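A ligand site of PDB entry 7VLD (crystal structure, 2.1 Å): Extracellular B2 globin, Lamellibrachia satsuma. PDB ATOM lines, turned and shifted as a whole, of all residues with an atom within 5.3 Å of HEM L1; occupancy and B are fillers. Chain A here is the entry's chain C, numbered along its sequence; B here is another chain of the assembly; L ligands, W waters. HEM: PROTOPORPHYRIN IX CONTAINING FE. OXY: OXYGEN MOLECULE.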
ATOM      1  N   LEU A  40       6.394  -8.498 -13.764  1.00  0.00           N
ATOM      2  CA  LEU A  40       7.457  -8.646 -14.747  1.00  0.00           C
ATOM      3  C   LEU A  40       8.604  -7.686 -14.467  1.00  0.00           C
ATOM      4  O   LEU A  40       9.788  -8.082 -14.494  1.00  0.00           O
ATOM      5  CB  LEU A  40       6.894  -8.406 -16.149  1.00  0.00           C
ATOM      6  CG  LEU A  40       7.882  -8.415 -17.321  1.00  0.00           C
ATOM      7  CD1 LEU A  40       8.487  -9.797 -17.491  1.00  0.00           C
ATOM      8  CD2 LEU A  40       7.206  -7.958 -18.604  1.00  0.00           C
ATOM      9  N   LEU A  50      12.012  -1.300 -22.215  1.00  0.00           N
ATOM     10  CA  LEU A  50      11.383  -1.639 -23.493  1.00  0.00           C
ATOM     11  C   LEU A  50      10.070  -0.896 -23.706  1.00  0.00           C
ATOM     12  O   LEU A  50       9.567  -0.861 -24.829  1.00  0.00           O
ATOM     13  CB  LEU A  50      11.138  -3.153 -23.566  1.00  0.00           C
ATOM     14  CG  LEU A  50      12.371  -4.031 -23.328  1.00  0.00           C
ATOM     15  CD1 LEU A  50      11.983  -5.494 -23.319  1.00  0.00           C
ATOM     16  CD2 LEU A  50      13.427  -3.749 -24.379  1.00  0.00           C
ATOM     17  N   PHE A  51       9.509  -0.309 -22.649  1.00  0.00           N
ATOM     18  CA  PHE A  51       8.212   0.346 -22.695  1.00  0.00           C
ATOM     19  C   PHE A  51       8.330   1.837 -22.418  1.00  0.00           C
ATOM     20  O   PHE A  51       7.470   2.453 -21.785  1.00  0.00           O
ATOM     21  CB  PHE A  51       7.243  -0.316 -21.707  1.00  0.00           C
ATOM     22  CG  PHE A  51       7.125  -1.799 -21.886  1.00  0.00           C
ATOM     23  CD1 PHE A  51       6.255  -2.334 -22.820  1.00  0.00           C
ATOM     24  CD2 PHE A  51       7.892  -2.664 -21.111  1.00  0.00           C
ATOM     25  CE1 PHE A  51       6.159  -3.702 -22.990  1.00  0.00           C
ATOM     26  CE2 PHE A  51       7.794  -4.040 -21.274  1.00  0.00           C
ATOM     27  CZ  PHE A  51       6.921  -4.554 -22.218  1.00  0.00           C
ATOM     28  N   ARG A  53       8.164   4.184 -24.698  1.00  0.00           N
ATOM     29  CA  ARG A  53       7.181   4.897 -25.508  1.00  0.00           C
ATOM     30  C   ARG A  53       5.806   4.910 -24.873  1.00  0.00           C
ATOM     31  O   ARG A  53       5.005   5.803 -25.180  1.00  0.00           O
ATOM     32  CB  ARG A  53       7.116   4.277 -26.904  1.00  0.00           C
ATOM     33  CG  ARG A  53       6.496   5.189 -27.955  1.00  0.00           C
ATOM     34  CD  ARG A  53       6.038   4.402 -29.174  1.00  0.00           C
ATOM     35  NE  ARG A  53       4.889   3.556 -28.857  1.00  0.00           N
ATOM     36  CZ  ARG A  53       3.632   3.957 -28.877  1.00  0.00           C
ATOM     37  NH1 ARG A  53       2.653   3.118 -28.572  1.00  0.00           N
ATOM     38  NH2 ARG A  53       3.335   5.214 -29.205  1.00  0.00           N
ATOM     39  N   VAL A  54       5.500   3.954 -24.000  1.00  0.00           N
ATOM     40  CA  VAL A  54       4.199   3.873 -23.352  1.00  0.00           C
ATOM     41  C   VAL A  54       4.308   4.155 -21.852  1.00  0.00           C
ATOM     42  O   VAL A  54       3.431   3.756 -21.093  1.00  0.00           O
ATOM     43  CB  VAL A  54       3.527   2.511 -23.623  1.00  0.00           C
ATOM     44  CG1 VAL A  54       3.273   2.342 -25.108  1.00  0.00           C
ATOM     45  CG2 VAL A  54       4.387   1.382 -23.085  1.00  0.00           C
ATOM     46  N   HIS A  67      -1.699   0.945 -23.026  1.00  0.00           N
ATOM     47  CA  HIS A  67      -0.895  -0.189 -23.450  1.00  0.00           C
ATOM     48  C   HIS A  67      -1.370  -1.475 -22.788  1.00  0.00           C
ATOM     49  O   HIS A  67      -1.494  -2.512 -23.451  1.00  0.00           O
ATOM     50  CB  HIS A  67       0.575   0.062 -23.133  1.00  0.00           C
ATOM     51  CG  HIS A  67       1.446  -1.149 -23.290  1.00  0.00           C
ATOM     52  ND1 HIS A  67       1.784  -1.664 -24.520  1.00  0.00           N
ATOM     53  CD2 HIS A  67       2.030  -1.952 -22.374  1.00  0.00           C
ATOM     54  CE1 HIS A  67       2.549  -2.735 -24.354  1.00  0.00           C
ATOM     55  NE2 HIS A  67       2.712  -2.927 -23.058  1.00  0.00           N
ATOM     56  N   ARG A  70      -4.345  -2.758 -24.442  1.00  0.00           N
ATOM     57  CA  ARG A  70      -4.007  -3.343 -25.731  1.00  0.00           C
ATOM     58  C   ARG A  70      -3.474  -4.769 -25.567  1.00  0.00           C
ATOM     59  O   ARG A  70      -3.877  -5.681 -26.291  1.00  0.00           O
ATOM     60  CB  ARG A  70      -2.986  -2.480 -26.475  1.00  0.00           C
ATOM     61  CG  ARG A  70      -3.565  -1.242 -27.137  1.00  0.00           C
ATOM     62  CD  ARG A  70      -2.609  -0.616 -28.138  1.00  0.00           C
ATOM     63  NE  ARG A  70      -1.409  -0.069 -27.503  1.00  0.00           N
ATOM     64  CZ  ARG A  70      -1.334   1.154 -26.987  1.00  0.00           C
ATOM     65  NH1 ARG A  70      -2.376   1.960 -27.031  1.00  0.00           N
ATOM     66  NH2 ARG A  70      -0.199   1.555 -26.424  1.00  0.00           N
ATOM     67  N   VAL A  71      -2.550  -4.960 -24.625  1.00  0.00           N
ATOM     68  CA  VAL A  71      -1.998  -6.292 -24.384  1.00  0.00           C
ATOM     69  C   VAL A  71      -3.103  -7.256 -23.954  1.00  0.00           C
ATOM     70  O   VAL A  71      -3.196  -8.384 -24.450  1.00  0.00           O
ATOM     71  CB  VAL A  71      -0.874  -6.227 -23.330  1.00  0.00           C
ATOM     72  CG1 VAL A  71      -0.382  -7.620 -22.980  1.00  0.00           C
ATOM     73  CG2 VAL A  71       0.270  -5.351 -23.827  1.00  0.00           C
ATOM     74  N   GLY A  74      -5.142  -8.148 -26.805  1.00  0.00           N
ATOM     75  CA  GLY A  74      -4.462  -9.133 -27.634  1.00  0.00           C
ATOM     76  C   GLY A  74      -4.546 -10.532 -27.056  1.00  0.00           C
ATOM     77  O   GLY A  74      -4.750 -11.502 -27.792  1.00  0.00           O
ATOM     78  N   LEU A  75      -4.373 -10.664 -25.738  1.00  0.00           N
ATOM     79  CA  LEU A  75      -4.489 -11.984 -25.115  1.00  0.00           C
ATOM     80  C   LEU A  75      -5.928 -12.492 -25.189  1.00  0.00           C
ATOM     81  O   LEU A  75      -6.148 -13.686 -25.421  1.00  0.00           O
ATOM     82  CB  LEU A  75      -4.008 -11.926 -23.662  1.00  0.00           C
ATOM     83  CG  LEU A  75      -3.974 -13.290 -22.964  1.00  0.00           C
ATOM     84  CD1 LEU A  75      -3.066 -14.255 -23.714  1.00  0.00           C
ATOM     85  CD2 LEU A  75      -3.537 -13.164 -21.512  1.00  0.00           C
ATOM     86  N   LEU A  95       0.839 -10.542 -34.322  1.00  0.00           N
ATOM     87  CA  LEU A  95       1.419 -10.158 -33.042  1.00  0.00           C
ATOM     88  C   LEU A  95       2.937 -10.357 -33.038  1.00  0.00           C
ATOM     89  O   LEU A  95       3.655  -9.583 -32.406  1.00  0.00           O
ATOM     90  CB  LEU A  95       0.786 -10.951 -31.906  1.00  0.00           C
ATOM     91  CG  LEU A  95      -0.699 -10.676 -31.655  1.00  0.00           C
ATOM     92  CD1 LEU A  95      -1.277 -11.653 -30.652  1.00  0.00           C
ATOM     93  CD2 LEU A  95      -0.889  -9.245 -31.182  1.00  0.00           C
ATOM     94  N   GLN A  98       4.563  -7.415 -34.681  1.00  0.00           N
ATOM     95  CA  GLN A  98       4.453  -6.248 -33.820  1.00  0.00           C
ATOM     96  C   GLN A  98       5.518  -6.241 -32.726  1.00  0.00           C
ATOM     97  O   GLN A  98       5.986  -5.172 -32.323  1.00  0.00           O
ATOM     98  CB  GLN A  98       3.049  -6.172 -33.202  1.00  0.00           C
ATOM     99  CG  GLN A  98       1.967  -5.732 -34.155  1.00  0.00           C
ATOM    100  CD  GLN A  98       0.602  -5.660 -33.499  1.00  0.00           C
ATOM    101  OE1 GLN A  98       0.227  -6.553 -32.745  1.00  0.00           O
ATOM    102  NE2 GLN A  98      -0.139  -4.599 -33.773  1.00  0.00           N
ATOM    103  N   HIS A  99       5.896  -7.415 -32.240  1.00  0.00           N
ATOM    104  CA  HIS A  99       6.975  -7.545 -31.273  1.00  0.00           C
ATOM    105  C   HIS A  99       8.320  -7.818 -31.925  1.00  0.00           C
ATOM    106  O   HIS A  99       9.341  -7.867 -31.219  1.00  0.00           O
ATOM    107  CB  HIS A  99       6.667  -8.661 -30.272  1.00  0.00           C
ATOM    108  CG  HIS A  99       5.414  -8.431 -29.471  1.00  0.00           C
ATOM    109  ND1 HIS A  99       4.155  -8.666 -29.974  1.00  0.00           N
ATOM    110  CD2 HIS A  99       5.238  -7.984 -28.203  1.00  0.00           C
ATOM    111  CE1 HIS A  99       3.258  -8.377 -29.057  1.00  0.00           C
ATOM    112  NE2 HIS A  99       3.885  -7.964 -27.971  1.00  0.00           N
ATOM    113  N   ARG A 102      12.179  -5.481 -32.005  1.00  0.00           N
ATOM    114  CA  ARG A 102      12.397  -4.472 -30.969  1.00  0.00           C
ATOM    115  C   ARG A 102      13.488  -5.039 -30.073  1.00  0.00           C
ATOM    116  O   ARG A 102      13.234  -5.973 -29.310  1.00  0.00           O
ATOM    117  CB  ARG A 102      11.112  -4.195 -30.190  1.00  0.00           C
ATOM    118  CG  ARG A 102       9.911  -3.823 -31.043  1.00  0.00           C
ATOM    119  CD  ARG A 102       8.658  -3.779 -30.187  1.00  0.00           C
ATOM    120  NE  ARG A 102       7.488  -3.350 -30.941  1.00  0.00           N
ATOM    121  CZ  ARG A 102       7.091  -2.082 -31.050  1.00  0.00           C
ATOM    122  NH1 ARG A 102       6.007  -1.776 -31.757  1.00  0.00           N
ATOM    123  NH2 ARG A 102       7.772  -1.115 -30.448  1.00  0.00           N
ATOM    124  N   GLY A 104      15.354  -5.478 -27.332  1.00  0.00           N
ATOM    125  CA  GLY A 104      15.286  -6.271 -26.120  1.00  0.00           C
ATOM    126  C   GLY A 104      14.072  -7.156 -25.954  1.00  0.00           C
ATOM    127  O   GLY A 104      13.879  -7.700 -24.862  1.00  0.00           O
ATOM    128  N   VAL A 105      13.249  -7.330 -26.983  1.00  0.00           N
ATOM    129  CA  VAL A 105      12.077  -8.202 -26.910  1.00  0.00           C
ATOM    130  C   VAL A 105      12.502  -9.589 -27.395  1.00  0.00           C
ATOM    131  O   VAL A 105      12.695  -9.807 -28.596  1.00  0.00           O
ATOM    132  CB  VAL A 105      10.917  -7.655 -27.744  1.00  0.00           C
ATOM    133  CG1 VAL A 105       9.732  -8.594 -27.685  1.00  0.00           C
ATOM    134  CG2 VAL A 105      10.526  -6.270 -27.249  1.00  0.00           C
ATOM    135  N   THR A 106      12.651 -10.522 -26.457  1.00  0.00           N
ATOM    136  CA  THR A 106      13.199 -11.841 -26.728  1.00  0.00           C
ATOM    137  C   THR A 106      12.245 -12.916 -26.218  1.00  0.00           C
ATOM    138  O   THR A 106      11.226 -12.624 -25.591  1.00  0.00           O
ATOM    139  CB  THR A 106      14.577 -12.018 -26.088  1.00  0.00           C
ATOM    140  OG1 THR A 106      14.446 -11.992 -24.669  1.00  0.00           O
ATOM    141  CG2 THR A 106      15.525 -10.903 -26.528  1.00  0.00           C
ATOM    142  N   GLY A 109      11.912 -12.836 -22.342  1.00  0.00           N
ATOM    143  CA  GLY A 109      10.925 -11.946 -21.757  1.00  0.00           C
ATOM    144  C   GLY A 109       9.529 -12.542 -21.715  1.00  0.00           C
ATOM    145  O   GLY A 109       8.762 -12.284 -20.790  1.00  0.00           O
ATOM    146  N   PHE A 110       9.195 -13.357 -22.717  1.00  0.00           N
ATOM    147  CA  PHE A 110       7.887 -14.017 -22.730  1.00  0.00           C
ATOM    148  C   PHE A 110       7.822 -15.131 -21.694  1.00  0.00           C
ATOM    149  O   PHE A 110       6.765 -15.351 -21.085  1.00  0.00           O
ATOM    150  CB  PHE A 110       7.578 -14.551 -24.127  1.00  0.00           C
ATOM    151  CG  PHE A 110       7.014 -13.519 -25.062  1.00  0.00           C
ATOM    152  CD1 PHE A 110       7.841 -12.584 -25.673  1.00  0.00           C
ATOM    153  CD2 PHE A 110       5.657 -13.477 -25.331  1.00  0.00           C
ATOM    154  CE1 PHE A 110       7.324 -11.638 -26.534  1.00  0.00           C
ATOM    155  CE2 PHE A 110       5.135 -12.524 -26.188  1.00  0.00           C
ATOM    156  CZ  PHE A 110       5.963 -11.609 -26.789  1.00  0.00           C
ATOM    157  N   ILE A 113       7.111 -13.210 -18.464  1.00  0.00           N
ATOM    158  CA  ILE A 113       5.724 -12.783 -18.303  1.00  0.00           C
ATOM    159  C   ILE A 113       4.796 -13.977 -18.149  1.00  0.00           C
ATOM    160  O   ILE A 113       3.708 -13.835 -17.570  1.00  0.00           O
ATOM    161  CB  ILE A 113       5.295 -11.883 -19.485  1.00  0.00           C
ATOM    162  CG1 ILE A 113       4.163 -10.959 -19.043  1.00  0.00           C
ATOM    163  CG2 ILE A 113       4.861 -12.717 -20.673  1.00  0.00           C
ATOM    164  CD1 ILE A 113       3.684 -10.015 -20.136  1.00  0.00           C
ATOM    165  N   PHE A 117       1.955 -14.094 -15.193  1.00  0.00           N
ATOM    166  CA  PHE A 117       0.544 -14.480 -15.218  1.00  0.00           C
ATOM    167  C   PHE A 117       0.258 -15.598 -14.227  1.00  0.00           C
ATOM    168  O   PHE A 117      -0.767 -15.593 -13.548  1.00  0.00           O
ATOM    169  CB  PHE A 117       0.150 -14.910 -16.635  1.00  0.00           C
ATOM    170  CG  PHE A 117      -0.281 -13.774 -17.523  1.00  0.00           C
ATOM    171  CD1 PHE A 117      -1.592 -13.342 -17.528  1.00  0.00           C
ATOM    172  CD2 PHE A 117       0.628 -13.152 -18.364  1.00  0.00           C
ATOM    173  CE1 PHE A 117      -1.998 -12.293 -18.349  1.00  0.00           C
ATOM    174  CE2 PHE A 117       0.241 -12.118 -19.181  1.00  0.00           C
ATOM    175  CZ  PHE A 117      -1.079 -11.687 -19.175  1.00  0.00           C
ATOM    176  N   PHE A 137      -1.187 -21.042 -22.751  1.00  0.00           N
ATOM    177  CA  PHE A 137      -0.455 -19.777 -22.771  1.00  0.00           C
ATOM    178  C   PHE A 137       0.850 -19.928 -23.561  1.00  0.00           C
ATOM    179  O   PHE A 137       1.203 -19.058 -24.361  1.00  0.00           O
ATOM    180  CB  PHE A 137      -0.172 -19.313 -21.338  1.00  0.00           C
ATOM    181  CG  PHE A 137       0.360 -17.915 -21.251  1.00  0.00           C
ATOM    182  CD1 PHE A 137      -0.498 -16.832 -21.122  1.00  0.00           C
ATOM    183  CD2 PHE A 137       1.725 -17.671 -21.274  1.00  0.00           C
ATOM    184  CE1 PHE A 137      -0.018 -15.540 -21.031  1.00  0.00           C
ATOM    185  CE2 PHE A 137       2.221 -16.375 -21.188  1.00  0.00           C
ATOM    186  CZ  PHE A 137       1.344 -15.313 -21.057  1.00  0.00           C
ATOM    187  N   ILE A 140       0.241 -20.064 -27.199  1.00  0.00           N
ATOM    188  CA  ILE A 140       0.035 -18.726 -27.755  1.00  0.00           C
ATOM    189  C   ILE A 140       1.375 -18.002 -27.918  1.00  0.00           C
ATOM    190  O   ILE A 140       1.663 -17.435 -28.971  1.00  0.00           O
ATOM    191  CB  ILE A 140      -0.943 -17.927 -26.875  1.00  0.00           C
ATOM    192  CG1 ILE A 140      -2.362 -18.515 -27.011  1.00  0.00           C
ATOM    193  CG2 ILE A 140      -0.915 -16.451 -27.240  1.00  0.00           C
ATOM    194  CD1 ILE A 140      -3.377 -17.907 -26.078  1.00  0.00           C
ATOM    195  N   THR A 141       2.213 -18.032 -26.876  1.00  0.00           N
ATOM    196  CA  THR A 141       3.484 -17.316 -26.950  1.00  0.00           C
ATOM    197  C   THR A 141       4.446 -17.957 -27.935  1.00  0.00           C
ATOM    198  O   THR A 141       5.312 -17.264 -28.491  1.00  0.00           O
ATOM    199  CB  THR A 141       4.131 -17.224 -25.571  1.00  0.00           C
ATOM    200  OG1 THR A 141       4.344 -18.542 -25.036  1.00  0.00           O
ATOM    201  CG2 THR A 141       3.245 -16.436 -24.613  1.00  0.00           C
ATOM    202  N   MET A 144       3.757 -16.206 -30.969  1.00  0.00           N
ATOM    203  CA  MET A 144       4.125 -14.795 -30.891  1.00  0.00           C
ATOM    204  C   MET A 144       5.624 -14.575 -31.000  1.00  0.00           C
ATOM    205  O   MET A 144       6.053 -13.470 -31.348  1.00  0.00           O
ATOM    206  CB  MET A 144       3.619 -14.198 -29.568  1.00  0.00           C
ATOM    207  CG  MET A 144       2.107 -14.119 -29.444  1.00  0.00           C
ATOM    208  SD  MET A 144       1.597 -13.247 -27.950  1.00  0.00           S
ATOM    209  CE  MET A 144       2.300 -11.622 -28.240  1.00  0.00           C
ATOM    210  N   HIS B  90      -3.935   6.143 -30.671  1.00  0.00           N
ATOM    211  CA  HIS B  90      -3.214   4.984 -31.180  1.00  0.00           C
ATOM    212  C   HIS B  90      -3.879   4.438 -32.448  1.00  0.00           C
ATOM    213  O   HIS B  90      -3.201   4.170 -33.443  1.00  0.00           O
ATOM    214  CB  HIS B  90      -3.133   3.894 -30.101  1.00  0.00           C
ATOM    215  CG  HIS B  90      -2.259   2.740 -30.465  1.00  0.00           C
ATOM    216  ND1 HIS B  90      -0.891   2.780 -30.360  1.00  0.00           N
ATOM    217  CD2 HIS B  90      -2.564   1.509 -30.944  1.00  0.00           C
ATOM    218  CE1 HIS B  90      -0.383   1.632 -30.745  1.00  0.00           C
ATOM    219  NE2 HIS B  90      -1.374   0.829 -31.106  1.00  0.00           N
ATOM    220  N   GLN B  94      -2.521   4.190 -36.384  1.00  0.00           N
ATOM    221  CA  GLN B  94      -2.623   2.937 -37.120  1.00  0.00           C
ATOM    222  C   GLN B  94      -3.320   3.085 -38.454  1.00  0.00           C
ATOM    223  O   GLN B  94      -3.249   2.174 -39.279  1.00  0.00           O
ATOM    224  CB  GLN B  94      -3.345   1.888 -36.269  1.00  0.00           C
ATOM    225  CG  GLN B  94      -2.567   1.399 -35.062  1.00  0.00           C
ATOM    226  CD  GLN B  94      -3.370   0.465 -34.175  1.00  0.00           C
ATOM    227  OE1 GLN B  94      -4.578   0.623 -34.034  1.00  0.00           O
ATOM    228  NE2 GLN B  94      -2.704  -0.525 -33.595  1.00  0.00           N
HETATM  229  CHA HEM L   1       3.121  -4.042 -27.693  1.00  0.00           C
HETATM  230  CHB HEM L   1       0.485  -8.041 -26.868  1.00  0.00           C
HETATM  231  CHC HEM L   1       4.075  -9.892 -24.164  1.00  0.00           C
HETATM  232  CHD HEM L   1       6.923  -6.193 -25.540  1.00  0.00           C
HETATM  233  C1A HEM L   1       2.080  -4.942 -27.682  1.00  0.00           C
HETATM  234  C2A HEM L   1       0.765  -4.751 -28.272  1.00  0.00           C
HETATM  235  C3A HEM L   1       0.044  -5.859 -28.051  1.00  0.00           C
HETATM  236  C4A HEM L   1       0.872  -6.790 -27.298  1.00  0.00           C
HETATM  237  CMA HEM L   1      -1.412  -6.103 -28.490  1.00  0.00           C
HETATM  238  CAA HEM L   1       0.256  -3.508 -29.041  1.00  0.00           C
HETATM  239  CBA HEM L   1       0.892  -3.425 -30.421  1.00  0.00           C
HETATM  240  CGA HEM L   1       0.252  -2.303 -31.211  1.00  0.00           C
HETATM  241  O1A HEM L   1      -0.928  -1.979 -30.945  1.00  0.00           O
HETATM  242  O2A HEM L   1       0.929  -1.741 -32.101  1.00  0.00           O
HETATM  243  C1B HEM L   1       1.215  -8.887 -26.040  1.00  0.00           C
HETATM  244  C2B HEM L   1       0.749 -10.144 -25.493  1.00  0.00           C
HETATM  245  C3B HEM L   1       1.749 -10.657 -24.733  1.00  0.00           C
HETATM  246  C4B HEM L   1       2.866  -9.734 -24.801  1.00  0.00           C
HETATM  247  CMB HEM L   1      -0.666 -10.708 -25.767  1.00  0.00           C
HETATM  248  CAB HEM L   1       1.796 -11.976 -23.924  1.00  0.00           C
HETATM  249  CBB HEM L   1       0.870 -12.936 -23.954  1.00  0.00           C
HETATM  250  C1C HEM L   1       5.173  -9.063 -24.307  1.00  0.00           C
HETATM  251  C2C HEM L   1       6.481  -9.245 -23.695  1.00  0.00           C
HETATM  252  C3C HEM L   1       7.273  -8.223 -24.075  1.00  0.00           C
HETATM  253  C4C HEM L   1       6.484  -7.365 -24.938  1.00  0.00           C
HETATM  254  CMC HEM L   1       6.825 -10.442 -22.782  1.00  0.00           C
HETATM  255  CAC HEM L   1       8.750  -7.920 -23.730  1.00  0.00           C
HETATM  256  CBC HEM L   1       9.538  -8.690 -22.968  1.00  0.00           C
HETATM  257  C1D HEM L   1       6.135  -5.271 -26.201  1.00  0.00           C
HETATM  258  C2D HEM L   1       6.565  -3.967 -26.664  1.00  0.00           C
HETATM  259  C3D HEM L   1       5.529  -3.370 -27.257  1.00  0.00           C
HETATM  260  C4D HEM L   1       4.394  -4.277 -27.193  1.00  0.00           C
HETATM  261  CMD HEM L   1       7.990  -3.373 -26.505  1.00  0.00           C
HETATM  262  CAD HEM L   1       5.547  -1.964 -27.893  1.00  0.00           C
HETATM  263  CBD HEM L   1       4.709  -1.024 -27.029  1.00  0.00           C
HETATM  264  CGD HEM L   1       4.515   0.290 -27.755  1.00  0.00           C
HETATM  265  O1D HEM L   1       5.488   1.077 -27.820  1.00  0.00           O
HETATM  266  O2D HEM L   1       3.396   0.531 -28.245  1.00  0.00           O
HETATM  267  NA  HEM L   1       2.098  -6.194 -27.094  1.00  0.00           N
HETATM  268  NB  HEM L   1       2.506  -8.667 -25.603  1.00  0.00           N
HETATM  269  NC  HEM L   1       5.219  -7.900 -25.059  1.00  0.00           N
HETATM  270  ND  HEM L   1       4.812  -5.418 -26.539  1.00  0.00           N
HETATM  271 FE   HEM L   1       3.673  -7.087 -26.123  1.00  0.00          FE
HETATM  272  O1  OXY L   2       3.398  -6.408 -24.473  1.00  0.00           O
HETATM  273  O2  OXY L   2       3.690  -5.454 -23.786  1.00  0.00           O
HETATM  274  O   HOH W   1       1.363  -0.693 -26.699  1.00  0.00           O
HETATM  275  O   HOH W   2       7.605   1.319 -25.678  1.00  0.00           O
HETATM  276  O   HOH W   3      -4.583  -5.039 -28.760  1.00  0.00           O
HETATM  277  O   HOH W   4      -3.113  -3.621 -30.444  1.00  0.00           O
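NE2 of His 67 lies within hydrogen-bond range of O2 of OXY L2 (2.8 Å).
An iron atom (FE) of HEM L1 is bound by a ring nitrogen (NE2) of His 99 (2.1 Å).
O1A of HEM L1 sits at hydrogen-bond distance from NE2 of His 90 of chain B (2.8 Å).
O2D of HEM L1 lies within salt-bridge range of NH1 of Arg 53 (2.7 Å).
O2A of HEM L1 sits close to NE2 of Gln 98, 3.5 Å away.
An oxygen (O1A) of HEM L1 is in salt-bridge range of the guanidinium group (NE) of Arg 70, at 3.97 Å.
FE of HEM L1 is bound by O1 of OXY L2, at 1.8 Å.
NE2 of Gln 94 of chain B is in hydrogen-bond range of NE2 of His 90 of chain B, 3.1 Å away.
NE of Arg 102 lies within hydrogen-bond range of O of Gln 98 (2.7 Å).
O of Leu 95 lies within hydrogen-bond range of ND1 of His 99 (2.6 Å).
The backbone carbonyl oxygen of Phe 137 is in hydrogen-bond range of the side-chain hydroxyl of Thr 141 (3.3 Å).
Residues that only touch HEM L1: Leu 50, Phe 51, Val 54, His 67, Val 71, Leu 75, Arg 102, Val 105, Gly 109, Phe 110, Ile 113, Phe 137, Met 144 and Gln 94 of chain B.
Within 4 Å of HEM L1: Leu 50, Phe 51, Arg 53, Val 54, His 67, Arg 70, Val 71, Leu 75, Gln 98, His 99, Arg 102, Val 105, Gly 109, Phe 110, Ile 113, Phe 137, Met 144, His 90 of chain B and Gln 94 of chain B.
Water W1 lies within hydrogen-bond range of a ring nitrogen (ND1) of His 67, the guanidinium group (NH2) of Arg 70 and an oxygen (O2D) of HEM L1.
Water W2 lies within hydrogen-bond range of O1D of HEM L1, O of Leu 50 and N of Arg 53.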
